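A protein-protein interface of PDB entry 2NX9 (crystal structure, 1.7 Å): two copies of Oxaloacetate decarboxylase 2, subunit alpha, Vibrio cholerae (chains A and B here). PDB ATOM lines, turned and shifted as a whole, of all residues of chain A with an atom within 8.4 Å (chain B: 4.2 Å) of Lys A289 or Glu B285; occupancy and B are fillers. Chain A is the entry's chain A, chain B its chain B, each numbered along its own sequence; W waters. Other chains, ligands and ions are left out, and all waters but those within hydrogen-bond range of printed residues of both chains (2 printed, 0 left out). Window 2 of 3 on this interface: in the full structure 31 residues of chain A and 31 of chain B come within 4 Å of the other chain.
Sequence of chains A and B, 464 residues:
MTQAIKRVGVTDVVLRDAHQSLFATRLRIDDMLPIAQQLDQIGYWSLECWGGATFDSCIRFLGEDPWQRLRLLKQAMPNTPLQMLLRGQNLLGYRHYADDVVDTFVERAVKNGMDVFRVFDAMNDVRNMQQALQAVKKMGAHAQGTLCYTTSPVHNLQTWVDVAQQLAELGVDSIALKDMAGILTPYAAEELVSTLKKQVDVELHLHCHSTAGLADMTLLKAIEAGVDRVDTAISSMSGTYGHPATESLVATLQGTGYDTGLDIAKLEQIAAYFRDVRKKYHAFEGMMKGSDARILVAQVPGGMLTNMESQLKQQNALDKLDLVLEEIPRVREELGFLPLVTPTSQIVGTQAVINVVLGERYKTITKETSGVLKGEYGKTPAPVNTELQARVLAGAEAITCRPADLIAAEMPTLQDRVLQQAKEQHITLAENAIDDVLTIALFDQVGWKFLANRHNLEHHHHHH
The backbone carbonyl oxygen (O) of Ser B236 is in hydrogen-bond range of the guanidinium group (NH1) of Arg B278.
The guanidinium group of Arg B278 is in salt-bridge range of the side-chain carboxylate of Glu B285, 2.7 Å away.
Among the printed residues, merely in contact across the chains: Lys A289 with Ser B235 (3.9 Å), Lys A289 with Ser B236 (3.8 Å), Lys A289 with Arg B278 (3.5 Å), Lys A289 with Glu B285 (3.7 Å), Gly A290 with Ser B235 (3.8 Å), Ser A291 with Ser B235 (3.5 Å) and Ala A293 with Ser B235 (3.5 Å).
Of chain B, only Ser B235, Ser B236, Arg B278 and Glu B285 come within 4 Å of Lys A289.
Of chain A, only Lys A289 (3.7 Å) comes within 4 Å of Glu B285.
No residue of chain A comes within 4 Å of Gly B286.
Of the printed residues of chain B, Ser A291 touches Ser B235.
Printed residues of chain A within 4 Å of Ser B235: Lys A289 (3.9 Å), Gly A290 (3.8 Å), Ser A291 (3.5 Å) and Ala A293 (3.5 Å).
Gly A286 touches none of the printed residues of chain B.
The nearest printed residue of chain A that does not touch Glu B285 is Gly A290 (8.2 Å).
Of the 11 printed residues of chain B, 4 touch a printed residue of chain A.
Printed residues of chain A that touch a printed residue of chain B: Lys A289, Gly A290, Ser A291 and Ala A293.
Hydrophobic or aromatic side chains of chain A within 4 Å of the printed part of chain B: Ala A293.
Among the printed residues, 7 pairs touch across the chains.
Among the printed residues, no Asp or Glu carboxylate lies within 4 Å of a Lys or Arg side-chain nitrogen of the other chain.
Positions printed for both chains: 285, 286 and 287.
Water W2 lies within hydrogen-bond range of the side-chain hydroxyl (OG) of Ser B235 (2.7 Å) and the backbone NH (N) of Ala A293 (3.0 Å).
Water W1 bridges the side-chain amino group (NZ) of Lys A289 (3.1 Å) and a ring nitrogen (ND1) of His B282 (3.5 Å).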
ATOM      1  N   THR A 211       3.537  11.939  -4.642  1.00  0.00           N
ATOM      2  CA  THR A 211       3.079  10.993  -3.611  1.00  0.00           C
ATOM      3  C   THR A 211       2.271   9.840  -4.148  1.00  0.00           C
ATOM      4  O   THR A 211       2.355   8.702  -3.693  1.00  0.00           O
ATOM      5  CB  THR A 211       2.375  11.758  -2.495  1.00  0.00           C
ATOM      6  OG1 THR A 211       3.075  12.963  -2.264  1.00  0.00           O
ATOM      7  CG2 THR A 211       2.333  10.948  -1.205  1.00  0.00           C
ATOM      8  N   THR A 240       8.951  10.281  -4.075  1.00  0.00           N
ATOM      9  CA  THR A 240       8.036   9.985  -2.956  1.00  0.00           C
ATOM     10  C   THR A 240       7.088  11.104  -2.600  1.00  0.00           C
ATOM     11  O   THR A 240       6.223  11.542  -3.349  1.00  0.00           O
ATOM     12  CB  THR A 240       8.782   9.440  -1.729  1.00  0.00           C
ATOM     13  OG1 THR A 240       9.736  10.370  -1.256  1.00  0.00           O
ATOM     14  CG2 THR A 240       9.450   8.105  -2.035  1.00  0.00           C
ATOM     15  N   TYR A 241       7.271  11.645  -1.358  1.00  0.00           N
ATOM     16  CA  TYR A 241       6.399  12.652  -0.754  1.00  0.00           C
ATOM     17  C   TYR A 241       6.614  13.973  -1.415  1.00  0.00           C
ATOM     18  O   TYR A 241       5.822  14.903  -1.282  1.00  0.00           O
ATOM     19  CB  TYR A 241       6.710  12.812   0.736  1.00  0.00           C
ATOM     20  CG  TYR A 241       6.580  11.550   1.539  1.00  0.00           C
ATOM     21  CD1 TYR A 241       5.348  11.173   2.059  1.00  0.00           C
ATOM     22  CD2 TYR A 241       7.711  10.785   1.811  1.00  0.00           C
ATOM     23  CE1 TYR A 241       5.252  10.043   2.860  1.00  0.00           C
ATOM     24  CE2 TYR A 241       7.624   9.650   2.604  1.00  0.00           C
ATOM     25  CZ  TYR A 241       6.393   9.297   3.131  1.00  0.00           C
ATOM     26  OH  TYR A 241       6.306   8.189   3.928  1.00  0.00           O
ATOM     27  N   GLU A 285      12.940  10.903   7.684  1.00  0.00           N
ATOM     28  CA  GLU A 285      12.315  10.435   6.440  1.00  0.00           C
ATOM     29  C   GLU A 285      11.091   9.574   6.718  1.00  0.00           C
ATOM     30  O   GLU A 285      11.109   8.736   7.626  1.00  0.00           O
ATOM     31  CB  GLU A 285      13.310   9.625   5.611  1.00  0.00           C
ATOM     32  CG  GLU A 285      14.580  10.340   5.150  1.00  0.00           C
ATOM     33  CD  GLU A 285      14.602  10.740   3.672  1.00  0.00           C
ATOM     34  OE1 GLU A 285      13.562  10.716   2.975  1.00  0.00           O
ATOM     35  OE2 GLU A 285      15.695  11.079   3.198  1.00  0.00           O
ATOM     36  N   GLY A 286      10.045   9.735   5.913  1.00  0.00           N
ATOM     37  CA  GLY A 286       8.873   8.894   6.054  1.00  0.00           C
ATOM     38  C   GLY A 286       9.261   7.546   5.519  1.00  0.00           C
ATOM     39  O   GLY A 286      10.321   7.392   4.894  1.00  0.00           O
ATOM     40  N   MET A 287       8.381   6.577   5.763  1.00  0.00           N
ATOM     41  CA  MET A 287       8.602   5.184   5.497  1.00  0.00           C
ATOM     42  C   MET A 287       8.108   4.714   4.136  1.00  0.00           C
ATOM     43  O   MET A 287       8.252   3.533   3.781  1.00  0.00           O
ATOM     44  CB  MET A 287       7.880   4.429   6.582  1.00  0.00           C
ATOM     45  CG  MET A 287       8.273   4.976   7.952  1.00  0.00           C
ATOM     46  SD  MET A 287      10.007   4.593   8.242  1.00  0.00           S
ATOM     47  CE  MET A 287       9.769   2.839   8.499  1.00  0.00           C
ATOM     48  N   MET A 288       7.498   5.593   3.365  1.00  0.00           N
ATOM     49  CA  MET A 288       6.956   5.088   2.095  1.00  0.00           C
ATOM     50  C   MET A 288       8.041   4.899   1.030  1.00  0.00           C
ATOM     51  O   MET A 288       8.933   5.718   0.883  1.00  0.00           O
ATOM     52  CB  MET A 288       5.816   5.944   1.541  1.00  0.00           C
ATOM     53  CG  MET A 288       6.332   6.964   0.525  1.00  0.00           C
ATOM     54  SD  MET A 288       5.447   6.797  -1.021  1.00  0.00           S
ATOM     55  CE  MET A 288       3.936   7.473  -0.429  1.00  0.00           C
ATOM     56  N   LYS A 289       7.916   3.806   0.280  1.00  0.00           N
ATOM     57  CA  LYS A 289       8.792   3.545  -0.836  1.00  0.00           C
ATOM     58  C   LYS A 289       7.956   3.465  -2.108  1.00  0.00           C
ATOM     59  O   LYS A 289       6.839   2.911  -2.101  1.00  0.00           O
ATOM     60  CB  LYS A 289       9.611   2.298  -0.552  1.00  0.00           C
ATOM     61  CG  LYS A 289      10.512   2.490   0.651  1.00  0.00           C
ATOM     62  CD  LYS A 289      11.423   1.313   0.893  1.00  0.00           C
ATOM     63  CE  LYS A 289      12.375   1.583   2.066  1.00  0.00           C
ATOM     64  NZ  LYS A 289      13.079   2.899   1.909  1.00  0.00           N
ATOM     65  N   GLY A 290       8.460   4.096  -3.170  1.00  0.00           N
ATOM     66  CA  GLY A 290       7.768   4.132  -4.446  1.00  0.00           C
ATOM     67  C   GLY A 290       6.689   5.192  -4.432  1.00  0.00           C
ATOM     68  O   GLY A 290       6.985   6.390  -4.266  1.00  0.00           O
ATOM     69  N   SER A 291       5.435   4.792  -4.605  1.00  0.00           N
ATOM     70  CA  SER A 291       4.318   5.733  -4.487  1.00  0.00           C
ATOM     71  C   SER A 291       3.229   5.032  -3.701  1.00  0.00           C
ATOM     72  O   SER A 291       3.267   3.825  -3.509  1.00  0.00           O
ATOM     73  CB  SER A 291       3.838   6.227  -5.883  1.00  0.00           C
ATOM     74  OG  SER A 291       3.717   5.127  -6.783  1.00  0.00           O
ATOM     75  N   ASP A 292       2.253   5.823  -3.260  1.00  0.00           N
ATOM     76  CA  ASP A 292       1.204   5.334  -2.413  1.00  0.00           C
ATOM     77  C   ASP A 292      -0.071   5.331  -3.227  1.00  0.00           C
ATOM     78  O   ASP A 292      -0.664   6.370  -3.517  1.00  0.00           O
ATOM     79  CB  ASP A 292       1.075   6.237  -1.188  1.00  0.00           C
ATOM     80  CG  ASP A 292       0.131   5.700  -0.142  1.00  0.00           C
ATOM     81  OD1 ASP A 292      -0.516   4.647  -0.341  1.00  0.00           O
ATOM     82  OD2 ASP A 292       0.048   6.340   0.921  1.00  0.00           O
ATOM     83  N   ALA A 293      -0.486   4.133  -3.575  1.00  0.00           N
ATOM     84  CA  ALA A 293      -1.679   3.901  -4.360  1.00  0.00           C
ATOM     85  C   ALA A 293      -2.960   4.192  -3.583  1.00  0.00           C
ATOM     86  O   ALA A 293      -3.995   4.462  -4.192  1.00  0.00           O
ATOM     87  CB  ALA A 293      -1.687   2.478  -4.860  1.00  0.00           C
ATOM     88  N   LEU B  22      15.440  -4.003  -6.477  1.00  0.00           N
ATOM     89  CA  LEU B  22      15.241  -3.182  -5.278  1.00  0.00           C
ATOM     90  C   LEU B  22      15.818  -3.770  -3.991  1.00  0.00           C
ATOM     91  O   LEU B  22      16.243  -3.021  -3.117  1.00  0.00           O
ATOM     92  CB  LEU B  22      13.761  -2.895  -5.084  1.00  0.00           C
ATOM     93  CG  LEU B  22      13.086  -1.954  -6.093  1.00  0.00           C
ATOM     94  CD1 LEU B  22      11.609  -1.819  -5.792  1.00  0.00           C
ATOM     95  CD2 LEU B  22      13.727  -0.623  -5.991  1.00  0.00           C
ATOM     96  N   SER B 235       2.956  -0.681  -6.830  1.00  0.00           N
ATOM     97  CA  SER B 235       3.475   0.602  -6.355  1.00  0.00           C
ATOM     98  C   SER B 235       4.459   0.534  -5.192  1.00  0.00           C
ATOM     99  O   SER B 235       5.497   1.148  -5.270  1.00  0.00           O
ATOM    100  CB  SER B 235       2.338   1.562  -6.040  1.00  0.00           C
ATOM    101  OG  SER B 235       1.569   1.114  -4.958  1.00  0.00           O
ATOM    102  N   SER B 236       4.146  -0.241  -4.159  1.00  0.00           N
ATOM    103  CA  SER B 236       5.022  -0.361  -2.984  1.00  0.00           C
ATOM    104  C   SER B 236       6.336  -1.029  -3.336  1.00  0.00           C
ATOM    105  O   SER B 236       7.296  -0.948  -2.577  1.00  0.00           O
ATOM    106  CB  SER B 236       4.281  -1.064  -1.846  1.00  0.00           C
ATOM    107  OG  SER B 236       3.643  -2.213  -2.353  1.00  0.00           O
ATOM    108  N   ARG B 278       8.025  -5.835   1.848  1.00  0.00           N
ATOM    109  CA  ARG B 278       9.249  -5.100   1.509  1.00  0.00           C
ATOM    110  C   ARG B 278       9.975  -4.604   2.785  1.00  0.00           C
ATOM    111  O   ARG B 278      11.199  -4.509   2.786  1.00  0.00           O
ATOM    112  CB  ARG B 278       8.973  -3.969   0.513  1.00  0.00           C
ATOM    113  CG  ARG B 278      10.203  -3.184   0.080  1.00  0.00           C
ATOM    114  CD  ARG B 278       9.939  -2.155  -1.037  1.00  0.00           C
ATOM    115  NE  ARG B 278      11.147  -1.415  -1.401  1.00  0.00           N
ATOM    116  CZ  ARG B 278      11.199  -0.466  -2.332  1.00  0.00           C
ATOM    117  NH1 ARG B 278      10.109  -0.141  -3.031  1.00  0.00           N
ATOM    118  NH2 ARG B 278      12.336   0.161  -2.577  1.00  0.00           N
ATOM    119  N   TYR B 281      12.664  -6.836   4.106  1.00  0.00           N
ATOM    120  CA  TYR B 281      13.864  -6.954   3.272  1.00  0.00           C
ATOM    121  C   TYR B 281      14.703  -5.693   3.261  1.00  0.00           C
ATOM    122  O   TYR B 281      15.554  -5.499   2.403  1.00  0.00           O
ATOM    123  CB  TYR B 281      13.497  -7.395   1.840  1.00  0.00           C
ATOM    124  CG  TYR B 281      12.903  -8.795   1.721  1.00  0.00           C
ATOM    125  CD1 TYR B 281      13.709  -9.900   1.458  1.00  0.00           C
ATOM    126  CD2 TYR B 281      11.521  -9.008   1.850  1.00  0.00           C
ATOM    127  CE1 TYR B 281      13.137 -11.202   1.345  1.00  0.00           C
ATOM    128  CE2 TYR B 281      10.960 -10.276   1.739  1.00  0.00           C
ATOM    129  CZ  TYR B 281      11.773 -11.357   1.492  1.00  0.00           C
ATOM    130  OH  TYR B 281      11.207 -12.598   1.375  1.00  0.00           O
ATOM    131  N   HIS B 282      14.472  -4.837   4.253  1.00  0.00           N
ATOM    132  CA  HIS B 282      15.227  -3.588   4.447  1.00  0.00           C
ATOM    133  C   HIS B 282      16.756  -3.768   4.355  1.00  0.00           C
ATOM    134  O   HIS B 282      17.462  -2.913   3.796  1.00  0.00           O
ATOM    135  CB  HIS B 282      14.787  -2.989   5.794  1.00  0.00           C
ATOM    136  CG  HIS B 282      15.667  -1.900   6.317  1.00  0.00           C
ATOM    137  ND1 HIS B 282      15.716  -0.644   5.750  1.00  0.00           N
ATOM    138  CD2 HIS B 282      16.504  -1.867   7.383  1.00  0.00           C
ATOM    139  CE1 HIS B 282      16.554   0.113   6.435  1.00  0.00           C
ATOM    140  NE2 HIS B 282      17.044  -0.602   7.435  1.00  0.00           N
ATOM    141  N   ALA B 283      17.245  -4.891   4.880  1.00  0.00           N
ATOM    142  CA  ALA B 283      18.661  -5.264   4.862  1.00  0.00           C
ATOM    143  C   ALA B 283      19.309  -5.133   3.485  1.00  0.00           C
ATOM    144  O   ALA B 283      20.478  -4.748   3.367  1.00  0.00           O
ATOM    145  CB  ALA B 283      18.827  -6.698   5.387  1.00  0.00           C
ATOM    146  N   PHE B 284      18.543  -5.459   2.443  1.00  0.00           N
ATOM    147  CA  PHE B 284      19.067  -5.561   1.080  1.00  0.00           C
ATOM    148  C   PHE B 284      18.795  -4.378   0.157  1.00  0.00           C
ATOM    149  O   PHE B 284      19.177  -4.429  -1.017  1.00  0.00           O
ATOM    150  CB  PHE B 284      18.535  -6.835   0.428  1.00  0.00           C
ATOM    151  CG  PHE B 284      18.737  -8.052   1.271  1.00  0.00           C
ATOM    152  CD1 PHE B 284      20.017  -8.541   1.515  1.00  0.00           C
ATOM    153  CD2 PHE B 284      17.643  -8.729   1.820  1.00  0.00           C
ATOM    154  CE1 PHE B 284      20.197  -9.658   2.294  1.00  0.00           C
ATOM    155  CE2 PHE B 284      17.831  -9.856   2.615  1.00  0.00           C
ATOM    156  CZ  PHE B 284      19.092 -10.324   2.846  1.00  0.00           C
ATOM    157  N   GLU B 285      18.158  -3.334   0.702  1.00  0.00           N
ATOM    158  CA  GLU B 285      17.821  -2.106  -0.016  1.00  0.00           C
ATOM    159  C   GLU B 285      19.069  -1.295  -0.355  1.00  0.00           C
ATOM    160  O   GLU B 285      20.016  -1.256   0.413  1.00  0.00           O
ATOM    161  CB  GLU B 285      16.879  -1.241   0.838  1.00  0.00           C
ATOM    162  CG  GLU B 285      15.481  -1.843   1.037  1.00  0.00           C
ATOM    163  CD  GLU B 285      14.436  -1.383  -0.005  1.00  0.00           C
ATOM    164  OE1 GLU B 285      14.741  -0.617  -0.957  1.00  0.00           O
ATOM    165  OE2 GLU B 285      13.277  -1.800   0.151  1.00  0.00           O
ATOM    166  N   GLY B 286      19.065  -0.651  -1.510  1.00  0.00           N
ATOM    167  CA  GLY B 286      20.160   0.238  -1.889  1.00  0.00           C
ATOM    168  C   GLY B 286      20.000   1.598  -1.228  1.00  0.00           C
ATOM    169  O   GLY B 286      19.015   1.838  -0.545  1.00  0.00           O
ATOM    170  N   MET B 287      20.948   2.502  -1.457  1.00  0.00           N
ATOM    171  CA  MET B 287      21.002   3.757  -0.691  1.00  0.00           C
ATOM    172  C   MET B 287      20.485   4.960  -1.472  1.00  0.00           C
ATOM    173  O   MET B 287      20.498   6.098  -0.981  1.00  0.00           O
ATOM    174  CB  MET B 287      22.437   4.065  -0.246  1.00  0.00           C
ATOM    175  CG  MET B 287      23.017   3.170   0.848  1.00  0.00           C
ATOM    176  SD  MET B 287      22.027   3.080   2.348  1.00  0.00           S
ATOM    177  CE  MET B 287      21.317   1.454   2.216  1.00  0.00           C
HETATM  178  O   HOH W   1      15.611   1.422   2.985  1.00  0.00           O
HETATM  179  O   HOH W   2       0.649   1.589  -2.515  1.00  0.00           O
